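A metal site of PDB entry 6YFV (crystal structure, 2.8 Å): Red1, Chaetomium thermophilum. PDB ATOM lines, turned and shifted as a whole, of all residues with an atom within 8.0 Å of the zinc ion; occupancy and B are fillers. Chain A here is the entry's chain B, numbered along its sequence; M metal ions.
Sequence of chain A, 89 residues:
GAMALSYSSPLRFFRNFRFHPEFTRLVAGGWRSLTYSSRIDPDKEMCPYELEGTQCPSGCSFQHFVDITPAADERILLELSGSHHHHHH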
ATOM      1  N   GLU A  45      17.103  22.748  -6.952  1.00  0.00           N
ATOM      2  CA  GLU A  45      18.531  22.944  -6.856  1.00  0.00           C
ATOM      3  C   GLU A  45      19.140  22.959  -8.248  1.00  0.00           C
ATOM      4  O   GLU A  45      18.724  22.194  -9.128  1.00  0.00           O
ATOM      5  CB  GLU A  45      19.182  21.864  -5.995  1.00  0.00           C
ATOM      6  CG  GLU A  45      18.403  21.621  -4.718  1.00  0.00           C
ATOM      7  CD  GLU A  45      18.907  20.454  -3.893  1.00  0.00           C
ATOM      8  OE1 GLU A  45      18.223  20.107  -2.899  1.00  0.00           O
ATOM      9  OE2 GLU A  45      19.976  19.888  -4.210  1.00  0.00           O
ATOM     10  N   MET A  46      20.099  23.856  -8.462  1.00  0.00           N
ATOM     11  CA  MET A  46      20.791  23.842  -9.747  1.00  0.00           C
ATOM     12  C   MET A  46      21.576  22.538  -9.898  1.00  0.00           C
ATOM     13  O   MET A  46      22.057  21.967  -8.916  1.00  0.00           O
ATOM     14  CB  MET A  46      21.715  25.058  -9.876  1.00  0.00           C
ATOM     15  CG  MET A  46      20.983  26.420  -9.874  1.00  0.00           C
ATOM     16  SD  MET A  46      19.598  26.478 -11.058  1.00  0.00           S
ATOM     17  CE  MET A  46      20.506  26.315 -12.590  1.00  0.00           C
ATOM     18  N   CYS A  47      21.656  22.049 -11.130  1.00  0.00           N
ATOM     19  CA  CYS A  47      22.290  20.758 -11.372  1.00  0.00           C
ATOM     20  C   CYS A  47      23.762  20.779 -10.980  1.00  0.00           C
ATOM     21  O   CYS A  47      24.523  21.609 -11.492  1.00  0.00           O
ATOM     22  CB  CYS A  47      22.171  20.347 -12.824  1.00  0.00           C
ATOM     23  SG  CYS A  47      22.874  18.717 -13.131  1.00  0.00           S
ATOM     24  N   PRO A  48      24.201  19.882 -10.098  1.00  0.00           N
ATOM     25  CA  PRO A  48      25.629  19.856  -9.755  1.00  0.00           C
ATOM     26  C   PRO A  48      26.493  19.319 -10.872  1.00  0.00           C
ATOM     27  O   PRO A  48      27.610  19.812 -11.066  1.00  0.00           O
ATOM     28  CB  PRO A  48      25.677  18.991  -8.492  1.00  0.00           C
ATOM     29  CG  PRO A  48      24.390  18.223  -8.490  1.00  0.00           C
ATOM     30  CD  PRO A  48      23.383  19.064  -9.190  1.00  0.00           C
ATOM     31  N   TYR A  49      25.999  18.366 -11.661  1.00  0.00           N
ATOM     32  CA  TYR A  49      26.784  17.921 -12.820  1.00  0.00           C
ATOM     33  C   TYR A  49      27.018  19.064 -13.799  1.00  0.00           C
ATOM     34  O   TYR A  49      28.166  19.310 -14.212  1.00  0.00           O
ATOM     35  CB  TYR A  49      26.106  16.723 -13.476  1.00  0.00           C
ATOM     36  CG  TYR A  49      25.599  15.725 -12.447  1.00  0.00           C
ATOM     37  CD1 TYR A  49      26.486  14.946 -11.698  1.00  0.00           C
ATOM     38  CD2 TYR A  49      24.239  15.589 -12.211  1.00  0.00           C
ATOM     39  CE1 TYR A  49      26.011  14.043 -10.733  1.00  0.00           C
ATOM     40  CE2 TYR A  49      23.762  14.698 -11.253  1.00  0.00           C
ATOM     41  CZ  TYR A  49      24.646  13.931 -10.525  1.00  0.00           C
ATOM     42  OH  TYR A  49      24.130  13.057  -9.581  1.00  0.00           O
ATOM     43  N   GLU A  50      25.956  19.800 -14.174  1.00  0.00           N
ATOM     44  CA  GLU A  50      26.128  20.905 -15.125  1.00  0.00           C
ATOM     45  C   GLU A  50      27.205  21.872 -14.652  1.00  0.00           C
ATOM     46  O   GLU A  50      28.114  22.213 -15.413  1.00  0.00           O
ATOM     47  CB  GLU A  50      24.798  21.645 -15.352  1.00  0.00           C
ATOM     48  CG  GLU A  50      24.854  22.713 -16.452  1.00  0.00           C
ATOM     49  CD  GLU A  50      23.493  23.330 -16.849  1.00  0.00           C
ATOM     50  OE1 GLU A  50      22.561  23.422 -16.009  1.00  0.00           O
ATOM     51  OE2 GLU A  50      23.369  23.728 -18.015  1.00  0.00           O
ATOM     52  N   LEU A  51      27.159  22.281 -13.371  1.00  0.00           N
ATOM     53  CA  LEU A  51      28.112  23.276 -12.878  1.00  0.00           C
ATOM     54  C   LEU A  51      29.531  22.722 -12.862  1.00  0.00           C
ATOM     55  O   LEU A  51      30.483  23.435 -13.219  1.00  0.00           O
ATOM     56  CB  LEU A  51      27.685  23.756 -11.492  1.00  0.00           C
ATOM     57  CG  LEU A  51      26.357  24.513 -11.549  1.00  0.00           C
ATOM     58  CD1 LEU A  51      25.632  24.624 -10.200  1.00  0.00           C
ATOM     59  CD2 LEU A  51      26.580  25.895 -12.146  1.00  0.00           C
ATOM     60  N   THR A  54      30.232  18.250 -16.176  1.00  0.00           N
ATOM     61  CA  THR A  54      30.148  16.842 -16.541  1.00  0.00           C
ATOM     62  C   THR A  54      28.713  16.490 -16.942  1.00  0.00           C
ATOM     63  O   THR A  54      27.753  17.129 -16.483  1.00  0.00           O
ATOM     64  CB  THR A  54      30.604  15.948 -15.391  1.00  0.00           C
ATOM     65  OG1 THR A  54      29.502  15.707 -14.517  1.00  0.00           O
ATOM     66  CG2 THR A  54      31.748  16.603 -14.622  1.00  0.00           C
ATOM     67  N   GLN A  55      28.560  15.494 -17.801  1.00  0.00           N
ATOM     68  CA  GLN A  55      27.290  15.309 -18.505  1.00  0.00           C
ATOM     69  C   GLN A  55      26.225  14.679 -17.611  1.00  0.00           C
ATOM     70  O   GLN A  55      26.442  13.613 -17.020  1.00  0.00           O
ATOM     71  CB  GLN A  55      27.514  14.458 -19.751  1.00  0.00           C
ATOM     72  CG  GLN A  55      26.250  13.864 -20.300  1.00  0.00           C
ATOM     73  CD  GLN A  55      26.456  13.202 -21.631  1.00  0.00           C
ATOM     74  OE1 GLN A  55      25.565  12.497 -22.123  1.00  0.00           O
ATOM     75  NE2 GLN A  55      27.622  13.422 -22.236  1.00  0.00           N
ATOM     76  N   CYS A  56      25.051  15.323 -17.520  1.00  0.00           N
ATOM     77  CA  CYS A  56      23.970  14.794 -16.690  1.00  0.00           C
ATOM     78  C   CYS A  56      23.595  13.394 -17.133  1.00  0.00           C
ATOM     79  O   CYS A  56      23.683  13.061 -18.315  1.00  0.00           O
ATOM     80  CB  CYS A  56      22.712  15.641 -16.733  1.00  0.00           C
ATOM     81  SG  CYS A  56      22.896  17.381 -16.564  1.00  0.00           S
ATOM     82  N   PRO A  57      23.134  12.565 -16.203  1.00  0.00           N
ATOM     83  CA  PRO A  57      22.483  11.322 -16.619  1.00  0.00           C
ATOM     84  C   PRO A  57      21.166  11.603 -17.321  1.00  0.00           C
ATOM     85  O   PRO A  57      20.597  12.699 -17.249  1.00  0.00           O
ATOM     86  CB  PRO A  57      22.289  10.563 -15.299  1.00  0.00           C
ATOM     87  CG  PRO A  57      22.615  11.525 -14.207  1.00  0.00           C
ATOM     88  CD  PRO A  57      23.536  12.544 -14.795  1.00  0.00           C
ATOM     89  N   SER A  58      20.691  10.612 -18.054  1.00  0.00           N
ATOM     90  CA  SER A  58      19.422  10.782 -18.735  1.00  0.00           C
ATOM     91  C   SER A  58      18.306  10.956 -17.719  1.00  0.00           C
ATOM     92  O   SER A  58      18.281  10.292 -16.681  1.00  0.00           O
ATOM     93  CB  SER A  58      19.140   9.587 -19.644  1.00  0.00           C
ATOM     94  OG  SER A  58      17.806   9.671 -20.121  1.00  0.00           O
ATOM     95  N   GLY A  59      17.392  11.882 -18.022  1.00  0.00           N
ATOM     96  CA  GLY A  59      16.267  12.179 -17.147  1.00  0.00           C
ATOM     97  C   GLY A  59      16.597  13.071 -15.963  1.00  0.00           C
ATOM     98  O   GLY A  59      15.704  13.280 -15.123  1.00  0.00           O
ATOM     99  N   CYS A  60      17.819  13.590 -15.867  1.00  0.00           N
ATOM    100  CA  CYS A  60      18.222  14.443 -14.760  1.00  0.00           C
ATOM    101  C   CYS A  60      17.204  15.538 -14.469  1.00  0.00           C
ATOM    102  O   CYS A  60      16.949  16.399 -15.309  1.00  0.00           O
ATOM    103  CB  CYS A  60      19.572  15.087 -15.080  1.00  0.00           C
ATOM    104  SG  CYS A  60      20.136  16.116 -13.746  1.00  0.00           S
ATOM    105  N   SER A  61      16.648  15.523 -13.254  1.00  0.00           N
ATOM    106  CA  SER A  61      15.589  16.454 -12.900  1.00  0.00           C
ATOM    107  C   SER A  61      16.054  17.596 -11.991  1.00  0.00           C
ATOM    108  O   SER A  61      15.223  18.259 -11.354  1.00  0.00           O
ATOM    109  CB  SER A  61      14.426  15.703 -12.262  1.00  0.00           C
ATOM    110  OG  SER A  61      14.714  15.336 -10.919  1.00  0.00           O
ATOM    111  N   PHE A  62      17.347  17.868 -11.916  1.00  0.00           N
ATOM    112  CA  PHE A  62      17.731  19.115 -11.268  1.00  0.00           C
ATOM    113  C   PHE A  62      17.319  20.294 -12.149  1.00  0.00           C
ATOM    114  O   PHE A  62      17.084  20.141 -13.360  1.00  0.00           O
ATOM    115  CB  PHE A  62      19.246  19.183 -11.052  1.00  0.00           C
ATOM    116  CG  PHE A  62      19.774  18.309  -9.950  1.00  0.00           C
ATOM    117  CD1 PHE A  62      19.888  18.803  -8.640  1.00  0.00           C
ATOM    118  CD2 PHE A  62      20.236  17.023 -10.222  1.00  0.00           C
ATOM    119  CE1 PHE A  62      20.427  18.015  -7.609  1.00  0.00           C
ATOM    120  CE2 PHE A  62      20.757  16.214  -9.219  1.00  0.00           C
ATOM    121  CZ  PHE A  62      20.861  16.726  -7.902  1.00  0.00           C
ATOM    122  N   GLN A  63      17.262  21.474 -11.552  1.00  0.00           N
ATOM    123  CA  GLN A  63      17.090  22.692 -12.341  1.00  0.00           C
ATOM    124  C   GLN A  63      18.347  22.925 -13.186  1.00  0.00           C
ATOM    125  O   GLN A  63      19.451  23.004 -12.645  1.00  0.00           O
ATOM    126  CB  GLN A  63      16.841  23.885 -11.426  1.00  0.00           C
ATOM    127  CG  GLN A  63      16.359  25.136 -12.130  1.00  0.00           C
ATOM    128  CD  GLN A  63      15.549  26.027 -11.210  1.00  0.00           C
ATOM    129  OE1 GLN A  63      14.383  26.340 -11.473  1.00  0.00           O
ATOM    130  NE2 GLN A  63      16.173  26.456 -10.111  1.00  0.00           N
ATOM    131  N   HIS A  64      18.182  23.026 -14.501  1.00  0.00           N
ATOM    132  CA  HIS A  64      19.298  23.341 -15.395  1.00  0.00           C
ATOM    133  C   HIS A  64      19.197  24.770 -15.922  1.00  0.00           C
ATOM    134  O   HIS A  64      18.131  25.383 -15.908  1.00  0.00           O
ATOM    135  CB  HIS A  64      19.346  22.343 -16.558  1.00  0.00           C
ATOM    136  CG  HIS A  64      19.537  20.938 -16.123  1.00  0.00           C
ATOM    137  ND1 HIS A  64      18.491  20.064 -15.966  1.00  0.00           N
ATOM    138  CD2 HIS A  64      20.651  20.260 -15.769  1.00  0.00           C
ATOM    139  CE1 HIS A  64      18.950  18.892 -15.544  1.00  0.00           C
ATOM    140  NE2 HIS A  64      20.258  18.987 -15.420  1.00  0.00           N
ATOM    141  N   PHE A  65      20.338  25.289 -16.391  1.00  0.00           N
ATOM    142  CA  PHE A  65      20.347  26.646 -16.938  1.00  0.00           C
ATOM    143  C   PHE A  65      19.397  26.794 -18.128  1.00  0.00           C
ATOM    144  O   PHE A  65      18.806  27.866 -18.317  1.00  0.00           O
ATOM    145  CB  PHE A  65      21.757  27.073 -17.365  1.00  0.00           C
ATOM    146  CG  PHE A  65      22.484  27.763 -16.286  1.00  0.00           C
ATOM    147  CD1 PHE A  65      22.387  29.137 -16.127  1.00  0.00           C
ATOM    148  CD2 PHE A  65      23.203  27.022 -15.368  1.00  0.00           C
ATOM    149  CE1 PHE A  65      23.031  29.750 -15.091  1.00  0.00           C
ATOM    150  CE2 PHE A  65      23.856  27.646 -14.332  1.00  0.00           C
ATOM    151  CZ  PHE A  65      23.774  29.006 -14.201  1.00  0.00           C
ATOM    152  N   ASP A  67      16.594  25.557 -18.344  1.00  0.00           N
ATOM    153  CA  ASP A  67      15.252  25.720 -17.802  1.00  0.00           C
ATOM    154  C   ASP A  67      14.947  27.178 -17.522  1.00  0.00           C
ATOM    155  O   ASP A  67      13.803  27.633 -17.708  1.00  0.00           O
ATOM    156  CB  ASP A  67      15.095  24.898 -16.518  1.00  0.00           C
ATOM    157  CG  ASP A  67      15.305  23.411 -16.741  1.00  0.00           C
ATOM    158  OD1 ASP A  67      14.970  22.928 -17.839  1.00  0.00           O
ATOM    159  OD2 ASP A  67      15.778  22.742 -15.780  1.00  0.00           O
HETATM  160 ZN    ZN M   1      21.620  17.601 -14.742  1.00  0.00          ZN
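The backbone NH (N) of His 64 sits at hydrogen-bond distance from the side-chain carboxylate (OD2) of Asp 67, 2.7 Å away. The side-chain sulfur (SG) of Cys 47 sits close to the backbone NH (N) of Glu 50 (3.4 Å). The backbone NH (N) of Cys 47 is in hydrogen-bond range of the backbone carbonyl oxygen (O) of Gln 63 (2.8 Å). The backbone NH (N) of Phe 62 lies close to the side-chain sulfur (SG) of Cys 60 (3.8 Å). SG of Cys 47 sits close to N of Tyr 49, at 3.5 Å. A ring nitrogen (ND1) of His 64 sits at hydrogen-bond distance from the backbone carbonyl oxygen of Phe 62, 3.0 Å away.
Within 4 Å of the zinc ion: Cys 47, Cys 56, Cys 60 and His 64.
The zinc ion is bound by NE2 of His 64 (2.1 Å), SG of Cys 56 (2.2 Å), SG of Cys 60 (2.3 Å) and SG of Cys 47 (2.3 Å). The zinc ion has four donor atoms within binding distance.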
